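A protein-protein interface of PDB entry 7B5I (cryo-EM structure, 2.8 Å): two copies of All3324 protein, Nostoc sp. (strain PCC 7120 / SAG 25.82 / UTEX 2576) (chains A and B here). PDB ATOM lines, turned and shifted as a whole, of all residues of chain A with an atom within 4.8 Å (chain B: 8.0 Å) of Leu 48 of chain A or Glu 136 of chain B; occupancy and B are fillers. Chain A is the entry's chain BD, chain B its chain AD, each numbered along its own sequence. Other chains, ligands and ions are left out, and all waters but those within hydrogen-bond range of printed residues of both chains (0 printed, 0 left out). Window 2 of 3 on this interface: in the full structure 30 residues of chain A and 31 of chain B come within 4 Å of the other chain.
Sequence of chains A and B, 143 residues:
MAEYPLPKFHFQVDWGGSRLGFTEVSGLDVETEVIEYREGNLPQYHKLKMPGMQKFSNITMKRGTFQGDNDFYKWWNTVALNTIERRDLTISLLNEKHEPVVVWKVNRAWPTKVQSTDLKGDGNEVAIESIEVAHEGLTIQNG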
ATOM      1  N   ILE A  35      30.246 -21.305   4.836  1.00  0.00           N
ATOM      2  CA  ILE A  35      31.108 -22.246   4.134  1.00  0.00           C
ATOM      3  C   ILE A  35      30.373 -23.573   4.034  1.00  0.00           C
ATOM      4  O   ILE A  35      29.743 -24.021   4.997  1.00  0.00           O
ATOM      5  CB  ILE A  35      32.468 -22.416   4.842  1.00  0.00           C
ATOM      6  CG1 ILE A  35      33.104 -21.055   5.097  1.00  0.00           C
ATOM      7  CG2 ILE A  35      33.399 -23.269   4.020  1.00  0.00           C
ATOM      8  CD1 ILE A  35      34.456 -21.125   5.755  1.00  0.00           C
ATOM      9  N   GLU A  36      30.462 -24.210   2.868  1.00  0.00           N
ATOM     10  CA  GLU A  36      29.706 -25.415   2.560  1.00  0.00           C
ATOM     11  C   GLU A  36      30.639 -26.592   2.312  1.00  0.00           C
ATOM     12  O   GLU A  36      31.769 -26.421   1.854  1.00  0.00           O
ATOM     13  CB  GLU A  36      28.814 -25.203   1.341  1.00  0.00           C
ATOM     14  CG  GLU A  36      27.780 -24.124   1.532  1.00  0.00           C
ATOM     15  CD  GLU A  36      26.895 -23.959   0.324  1.00  0.00           C
ATOM     16  OE1 GLU A  36      27.256 -24.478  -0.751  1.00  0.00           O
ATOM     17  OE2 GLU A  36      25.831 -23.317   0.447  1.00  0.00           O
ATOM     18  N   TYR A  37      30.149 -27.791   2.613  1.00  0.00           N
ATOM     19  CA  TYR A  37      30.988 -28.980   2.526  1.00  0.00           C
ATOM     20  C   TYR A  37      30.121 -30.220   2.354  1.00  0.00           C
ATOM     21  O   TYR A  37      29.058 -30.323   2.969  1.00  0.00           O
ATOM     22  CB  TYR A  37      31.862 -29.098   3.778  1.00  0.00           C
ATOM     23  CG  TYR A  37      32.835 -30.248   3.783  1.00  0.00           C
ATOM     24  CD1 TYR A  37      34.050 -30.148   3.133  1.00  0.00           C
ATOM     25  CD2 TYR A  37      32.555 -31.416   4.468  1.00  0.00           C
ATOM     26  CE1 TYR A  37      34.943 -31.183   3.143  1.00  0.00           C
ATOM     27  CE2 TYR A  37      33.445 -32.456   4.484  1.00  0.00           C
ATOM     28  CZ  TYR A  37      34.638 -32.333   3.820  1.00  0.00           C
ATOM     29  OH  TYR A  37      35.532 -33.368   3.832  1.00  0.00           O
ATOM     30  N   HIS A  46      22.464 -32.953  -0.033  1.00  0.00           N
ATOM     31  CA  HIS A  46      22.693 -31.522   0.084  1.00  0.00           C
ATOM     32  C   HIS A  46      23.780 -31.278   1.125  1.00  0.00           C
ATOM     33  O   HIS A  46      24.157 -32.174   1.879  1.00  0.00           O
ATOM     34  CB  HIS A  46      21.405 -30.755   0.419  1.00  0.00           C
ATOM     35  CG  HIS A  46      20.754 -31.156   1.706  1.00  0.00           C
ATOM     36  ND1 HIS A  46      20.043 -32.322   1.864  1.00  0.00           N
ATOM     37  CD2 HIS A  46      20.715 -30.532   2.907  1.00  0.00           C
ATOM     38  CE1 HIS A  46      19.591 -32.399   3.101  1.00  0.00           C
ATOM     39  NE2 HIS A  46      19.986 -31.325   3.756  1.00  0.00           N
ATOM     40  N   LYS A  47      24.282 -30.050   1.162  1.00  0.00           N
ATOM     41  CA  LYS A  47      25.546 -29.750   1.818  1.00  0.00           C
ATOM     42  C   LYS A  47      25.382 -29.344   3.279  1.00  0.00           C
ATOM     43  O   LYS A  47      24.299 -28.979   3.739  1.00  0.00           O
ATOM     44  CB  LYS A  47      26.281 -28.643   1.067  1.00  0.00           C
ATOM     45  CG  LYS A  47      26.611 -29.009  -0.352  1.00  0.00           C
ATOM     46  CD  LYS A  47      27.175 -27.843  -1.115  1.00  0.00           C
ATOM     47  CE  LYS A  47      27.279 -28.185  -2.584  1.00  0.00           C
ATOM     48  NZ  LYS A  47      27.487 -26.980  -3.426  1.00  0.00           N
ATOM     49  N   LEU A  48      26.498 -29.417   4.003  1.00  0.00           N
ATOM     50  CA  LEU A  48      26.625 -28.935   5.370  1.00  0.00           C
ATOM     51  C   LEU A  48      27.197 -27.524   5.373  1.00  0.00           C
ATOM     52  O   LEU A  48      27.973 -27.154   4.490  1.00  0.00           O
ATOM     53  CB  LEU A  48      27.532 -29.848   6.188  1.00  0.00           C
ATOM     54  CG  LEU A  48      27.284 -31.353   6.142  1.00  0.00           C
ATOM     55  CD1 LEU A  48      28.353 -32.060   6.931  1.00  0.00           C
ATOM     56  CD2 LEU A  48      25.915 -31.697   6.676  1.00  0.00           C
ATOM     57  N   LYS A  49      26.835 -26.752   6.397  1.00  0.00           N
ATOM     58  CA  LYS A  49      27.132 -25.327   6.461  1.00  0.00           C
ATOM     59  C   LYS A  49      27.760 -24.958   7.797  1.00  0.00           C
ATOM     60  O   LYS A  49      27.348 -25.456   8.846  1.00  0.00           O
ATOM     61  CB  LYS A  49      25.865 -24.512   6.253  1.00  0.00           C
ATOM     62  CG  LYS A  49      25.164 -24.811   4.953  1.00  0.00           C
ATOM     63  CD  LYS A  49      23.873 -24.049   4.860  1.00  0.00           C
ATOM     64  CE  LYS A  49      23.253 -24.199   3.498  1.00  0.00           C
ATOM     65  NZ  LYS A  49      22.864 -25.600   3.253  1.00  0.00           N
ATOM     66  N   MET A  50      28.749 -24.067   7.758  1.00  0.00           N
ATOM     67  CA  MET A  50      29.428 -23.633   8.968  1.00  0.00           C
ATOM     68  C   MET A  50      29.872 -22.178   8.824  1.00  0.00           C
ATOM     69  O   MET A  50      30.000 -21.672   7.704  1.00  0.00           O
ATOM     70  CB  MET A  50      30.627 -24.535   9.287  1.00  0.00           C
ATOM     71  CG  MET A  50      31.768 -24.408   8.317  1.00  0.00           C
ATOM     72  SD  MET A  50      33.177 -25.434   8.756  1.00  0.00           S
ATOM     73  CE  MET A  50      34.527 -24.286   8.535  1.00  0.00           C
ATOM     74  N   PHE B  56      17.919 -25.793  -0.445  1.00  0.00           N
ATOM     75  CA  PHE B  56      17.114 -25.177   0.599  1.00  0.00           C
ATOM     76  C   PHE B  56      17.474 -23.702   0.693  1.00  0.00           C
ATOM     77  O   PHE B  56      18.604 -23.308   0.404  1.00  0.00           O
ATOM     78  CB  PHE B  56      17.355 -25.854   1.954  1.00  0.00           C
ATOM     79  CG  PHE B  56      16.784 -27.235   2.065  1.00  0.00           C
ATOM     80  CD1 PHE B  56      15.834 -27.690   1.181  1.00  0.00           C
ATOM     81  CD2 PHE B  56      17.266 -28.109   3.012  1.00  0.00           C
ATOM     82  CE1 PHE B  56      15.327 -28.967   1.282  1.00  0.00           C
ATOM     83  CE2 PHE B  56      16.770 -29.388   3.107  1.00  0.00           C
ATOM     84  CZ  PHE B  56      15.802 -29.817   2.241  1.00  0.00           C
ATOM     85  N   SER B  57      16.517 -22.891   1.122  1.00  0.00           N
ATOM     86  CA  SER B  57      16.694 -21.448   1.174  1.00  0.00           C
ATOM     87  C   SER B  57      16.891 -20.964   2.604  1.00  0.00           C
ATOM     88  O   SER B  57      16.576 -21.659   3.572  1.00  0.00           O
ATOM     89  CB  SER B  57      15.489 -20.734   0.561  1.00  0.00           C
ATOM     90  OG  SER B  57      15.384 -21.017  -0.817  1.00  0.00           O
ATOM     91  N   ARG B  86      23.680 -23.918  17.593  1.00  0.00           N
ATOM     92  CA  ARG B  86      22.627 -24.277  16.657  1.00  0.00           C
ATOM     93  C   ARG B  86      21.374 -24.680  17.420  1.00  0.00           C
ATOM     94  O   ARG B  86      21.456 -25.244  18.513  1.00  0.00           O
ATOM     95  CB  ARG B  86      23.075 -25.415  15.743  1.00  0.00           C
ATOM     96  CG  ARG B  86      24.204 -25.053  14.799  1.00  0.00           C
ATOM     97  CD  ARG B  86      24.664 -26.270  14.027  1.00  0.00           C
ATOM     98  NE  ARG B  86      25.662 -25.957  13.012  1.00  0.00           N
ATOM     99  CZ  ARG B  86      26.973 -25.973  13.219  1.00  0.00           C
ATOM    100  NH1 ARG B  86      27.451 -26.280  14.412  1.00  0.00           N
ATOM    101  NH2 ARG B  86      27.806 -25.678  12.235  1.00  0.00           N
ATOM    102  N   ARG B  87      20.214 -24.379  16.842  1.00  0.00           N
ATOM    103  CA  ARG B  87      18.936 -24.615  17.497  1.00  0.00           C
ATOM    104  C   ARG B  87      17.968 -25.292  16.539  1.00  0.00           C
ATOM    105  O   ARG B  87      18.128 -25.220  15.322  1.00  0.00           O
ATOM    106  CB  ARG B  87      18.326 -23.311  18.010  1.00  0.00           C
ATOM    107  CG  ARG B  87      19.161 -22.582  19.034  1.00  0.00           C
ATOM    108  CD  ARG B  87      18.481 -21.301  19.444  1.00  0.00           C
ATOM    109  NE  ARG B  87      19.324 -20.475  20.293  1.00  0.00           N
ATOM    110  CZ  ARG B  87      19.017 -19.239  20.666  1.00  0.00           C
ATOM    111  NH1 ARG B  87      17.889 -18.687  20.258  1.00  0.00           N
ATOM    112  NH2 ARG B  87      19.839 -18.551  21.441  1.00  0.00           N
ATOM    113  N   LYS B 105       9.235 -27.775  10.350  1.00  0.00           N
ATOM    114  CA  LYS B 105      10.333 -28.138  11.235  1.00  0.00           C
ATOM    115  C   LYS B 105      11.644 -27.869  10.519  1.00  0.00           C
ATOM    116  O   LYS B 105      11.880 -28.408   9.432  1.00  0.00           O
ATOM    117  CB  LYS B 105      10.247 -29.604  11.646  1.00  0.00           C
ATOM    118  CG  LYS B 105       8.949 -29.963  12.311  1.00  0.00           C
ATOM    119  CD  LYS B 105       8.897 -31.428  12.659  1.00  0.00           C
ATOM    120  CE  LYS B 105       7.562 -31.787  13.281  1.00  0.00           C
ATOM    121  NZ  LYS B 105       7.471 -33.238  13.574  1.00  0.00           N
ATOM    122  N   VAL B 106      12.479 -27.028  11.122  1.00  0.00           N
ATOM    123  CA  VAL B 106      13.775 -26.679  10.559  1.00  0.00           C
ATOM    124  C   VAL B 106      14.863 -27.405  11.341  1.00  0.00           C
ATOM    125  O   VAL B 106      14.738 -27.604  12.550  1.00  0.00           O
ATOM    126  CB  VAL B 106      14.021 -25.160  10.621  1.00  0.00           C
ATOM    127  CG1 VAL B 106      15.194 -24.772   9.734  1.00  0.00           C
ATOM    128  CG2 VAL B 106      12.768 -24.406  10.202  1.00  0.00           C
ATOM    129  N   ASN B 107      15.929 -27.799  10.654  1.00  0.00           N
ATOM    130  CA  ASN B 107      17.022 -28.514  11.299  1.00  0.00           C
ATOM    131  C   ASN B 107      18.340 -27.748  11.273  1.00  0.00           C
ATOM    132  O   ASN B 107      18.748 -27.230  10.231  1.00  0.00           O
ATOM    133  CB  ASN B 107      17.203 -29.896  10.667  1.00  0.00           C
ATOM    134  CG  ASN B 107      18.064 -30.814  11.511  1.00  0.00           C
ATOM    135  OD1 ASN B 107      18.313 -30.545  12.687  1.00  0.00           O
ATOM    136  ND2 ASN B 107      18.522 -31.909  10.915  1.00  0.00           N
ATOM    137  N   ARG B 108      18.984 -27.672  12.435  1.00  0.00           N
ATOM    138  CA  ARG B 108      20.271 -26.997  12.602  1.00  0.00           C
ATOM    139  C   ARG B 108      20.303 -25.573  12.050  1.00  0.00           C
ATOM    140  O   ARG B 108      20.960 -25.311  11.042  1.00  0.00           O
ATOM    141  CB  ARG B 108      21.395 -27.820  11.959  1.00  0.00           C
ATOM    142  CG  ARG B 108      21.235 -29.323  12.110  1.00  0.00           C
ATOM    143  CD  ARG B 108      21.548 -29.775  13.524  1.00  0.00           C
ATOM    144  NE  ARG B 108      22.954 -29.567  13.854  1.00  0.00           N
ATOM    145  CZ  ARG B 108      23.515 -29.940  14.999  1.00  0.00           C
ATOM    146  NH1 ARG B 108      22.788 -30.543  15.930  1.00  0.00           N
ATOM    147  NH2 ARG B 108      24.802 -29.711  15.214  1.00  0.00           N
ATOM    148  N   ALA B 109      19.633 -24.643  12.721  1.00  0.00           N
ATOM    149  CA  ALA B 109      19.600 -23.260  12.246  1.00  0.00           C
ATOM    150  C   ALA B 109      20.410 -22.276  13.094  1.00  0.00           C
ATOM    151  O   ALA B 109      20.244 -22.205  14.311  1.00  0.00           O
ATOM    152  CB  ALA B 109      18.160 -22.783  12.115  1.00  0.00           C
ATOM    153  N   TRP B 110      21.287 -21.520  12.436  1.00  0.00           N
ATOM    154  CA  TRP B 110      22.099 -20.513  13.105  1.00  0.00           C
ATOM    155  C   TRP B 110      21.987 -19.192  12.356  1.00  0.00           C
ATOM    156  O   TRP B 110      21.871 -19.188  11.128  1.00  0.00           O
ATOM    157  CB  TRP B 110      23.570 -20.941  13.218  1.00  0.00           C
ATOM    158  CG  TRP B 110      24.186 -21.441  11.959  1.00  0.00           C
ATOM    159  CD1 TRP B 110      24.057 -22.684  11.428  1.00  0.00           C
ATOM    160  CD2 TRP B 110      25.047 -20.716  11.078  1.00  0.00           C
ATOM    161  NE1 TRP B 110      24.778 -22.781  10.268  1.00  0.00           N
ATOM    162  CE2 TRP B 110      25.395 -21.584  10.030  1.00  0.00           C
ATOM    163  CE3 TRP B 110      25.555 -19.417  11.072  1.00  0.00           C
ATOM    164  CZ2 TRP B 110      26.223 -21.195   8.987  1.00  0.00           C
ATOM    165  CZ3 TRP B 110      26.375 -19.033  10.036  1.00  0.00           C
ATOM    166  CH2 TRP B 110      26.702 -19.918   9.009  1.00  0.00           C
ATOM    167  N   VAL B 133      18.486 -16.522   8.677  1.00  0.00           N
ATOM    168  CA  VAL B 133      18.927 -17.773   9.283  1.00  0.00           C
ATOM    169  C   VAL B 133      19.194 -18.811   8.202  1.00  0.00           C
ATOM    170  O   VAL B 133      18.427 -18.940   7.241  1.00  0.00           O
ATOM    171  CB  VAL B 133      17.882 -18.320  10.278  1.00  0.00           C
ATOM    172  CG1 VAL B 133      18.301 -19.675  10.803  1.00  0.00           C
ATOM    173  CG2 VAL B 133      17.649 -17.347  11.415  1.00  0.00           C
ATOM    174  N   ALA B 134      20.271 -19.573   8.391  1.00  0.00           N
ATOM    175  CA  ALA B 134      20.639 -20.718   7.569  1.00  0.00           C
ATOM    176  C   ALA B 134      20.412 -22.008   8.345  1.00  0.00           C
ATOM    177  O   ALA B 134      20.494 -22.030   9.573  1.00  0.00           O
ATOM    178  CB  ALA B 134      22.102 -20.621   7.135  1.00  0.00           C
ATOM    179  N   HIS B 135      20.152 -23.092   7.621  1.00  0.00           N
ATOM    180  CA  HIS B 135      19.755 -24.348   8.242  1.00  0.00           C
ATOM    181  C   HIS B 135      20.169 -25.502   7.343  1.00  0.00           C
ATOM    182  O   HIS B 135      20.514 -25.305   6.176  1.00  0.00           O
ATOM    183  CB  HIS B 135      18.247 -24.375   8.486  1.00  0.00           C
ATOM    184  CG  HIS B 135      17.429 -24.266   7.235  1.00  0.00           C
ATOM    185  ND1 HIS B 135      17.007 -25.369   6.527  1.00  0.00           N
ATOM    186  CD2 HIS B 135      16.952 -23.189   6.571  1.00  0.00           C
ATOM    187  CE1 HIS B 135      16.311 -24.976   5.477  1.00  0.00           C
ATOM    188  NE2 HIS B 135      16.263 -23.658   5.481  1.00  0.00           N
ATOM    189  N   GLU B 136      20.126 -26.716   7.890  1.00  0.00           N
ATOM    190  CA  GLU B 136      20.364 -27.926   7.115  1.00  0.00           C
ATOM    191  C   GLU B 136      19.169 -28.866   7.187  1.00  0.00           C
ATOM    192  O   GLU B 136      19.336 -30.048   7.487  1.00  0.00           O
ATOM    193  CB  GLU B 136      21.600 -28.666   7.631  1.00  0.00           C
ATOM    194  CG  GLU B 136      22.888 -27.887   7.669  1.00  0.00           C
ATOM    195  CD  GLU B 136      23.951 -28.638   8.432  1.00  0.00           C
ATOM    196  OE1 GLU B 136      23.650 -29.744   8.915  1.00  0.00           O
ATOM    197  OE2 GLU B 136      25.079 -28.129   8.569  1.00  0.00           O
ATOM    198  N   GLY B 137      17.981 -28.371   6.877  1.00  0.00           N
ATOM    199  CA  GLY B 137      16.852 -29.235   6.599  1.00  0.00           C
ATOM    200  C   GLY B 137      15.527 -28.567   6.903  1.00  0.00           C
ATOM    201  O   GLY B 137      15.427 -27.672   7.742  1.00  0.00           O
ATOM    202  N   LEU B 138      14.488 -29.077   6.245  1.00  0.00           N
ATOM    203  CA  LEU B 138      13.137 -28.552   6.398  1.00  0.00           C
ATOM    204  C   LEU B 138      12.127 -29.653   6.112  1.00  0.00           C
ATOM    205  O   LEU B 138      12.314 -30.450   5.193  1.00  0.00           O
ATOM    206  CB  LEU B 138      12.890 -27.369   5.461  1.00  0.00           C
ATOM    207  CG  LEU B 138      11.502 -26.738   5.480  1.00  0.00           C
ATOM    208  CD1 LEU B 138      11.113 -26.307   6.873  1.00  0.00           C
ATOM    209  CD2 LEU B 138      11.474 -25.567   4.533  1.00  0.00           C
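The guanidinium group (NH2) of Arg 86 of chain B is in hydrogen-bond range of the backbone carbonyl oxygen (O) of Lys 49 of chain A (3.4 Å).
N of Lys 49 of chain A sits at hydrogen-bond distance from OE2 of Glu 136 of chain B, at 3.1 Å.
The backbone NH (N) of Trp 110 of chain B is in hydrogen-bond range of the backbone carbonyl oxygen (O) of Ala 134 of chain B.
O of Asn 107 of chain B is in hydrogen-bond range of N of Glu 136 of chain B, 2.8 Å away.
The backbone carbonyl oxygen of Ser 57 of chain B lies within hydrogen-bond range of a ring nitrogen (NE2) of His 135 of chain B (2.8 Å).
A ring nitrogen (ND1) of His 135 of chain B lies within hydrogen-bond range of the backbone carbonyl oxygen of Gly 137 of chain B, 3.0 Å away.
O of Tyr 37 of chain A sits at hydrogen-bond distance from N of Leu 48 of chain A (2.9 Å).
N of Ile 35 of chain A is in hydrogen-bond range of O of Met 50 of chain A, at 2.9 Å.
Among the printed residues, pairs that only touch across the chains: His 46 of chain A with Phe 56 of chain B (3.8 Å), His 46 of chain A with Glu 136 of chain B (3.997 Å), Leu 48 of chain A with Glu 136 of chain B (3.6 Å), Lys 49 of chain A with Trp 110 of chain B (3.97 Å), Lys 49 of chain A with His 135 of chain B (3.8 Å) and Met 50 of chain A with Trp 110 of chain B (3.8 Å).
Glu 36 of chain A touches none of the printed residues of chain B.
Of the printed residues of chain B, His 46 of chain A touches Phe 56 (3.8 Å) and Glu 136 (3.997 Å).
Printed residues of chain B within 4 Å of Leu 48 of chain A: Glu 136 (3.6 Å).
Printed residues of chain A within 4 Å of Phe 56 of chain B: His 46 (3.8 Å).
Printed residues of chain A within 4 Å of Arg 86 of chain B: Lys 49.
Val 106 of chain B touches none of the printed residues of chain A.
Printed residues of chain A within 4 Å of Trp 110 of chain B: Lys 49 and Met 50.
Of the printed residues of chain A, His 135 of chain B touches Lys 49 (3.8 Å).
Of the printed residues of chain A, Glu 136 of chain B touches His 46, Leu 48 and Lys 49.
The nearest residue of chain B that does not touch Leu 48 of chain A is His 135 of chain B (7.1 Å).
The nearest printed residue of chain A that does not touch Glu 136 of chain B is Lys 47 of chain A (4.3 Å).
The nearest printed residue of chain A that does not touch Arg 86 of chain B is Met 50 of chain A (4.2 Å).
Hydrophobic or aromatic side chains of chain B that line the printed part of chain A: Phe 56 and Trp 110.
Among the printed residues, 8 pairs touch across the chains.
Among the printed residues, no Asp or Glu carboxylate lies within 4 Å of a Lys or Arg side-chain nitrogen of the other chain.
No position is printed for both chains.
Of the 8 pairs that touch across the chains among the printed residues, none has its exchanged pair printed and touching as well.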
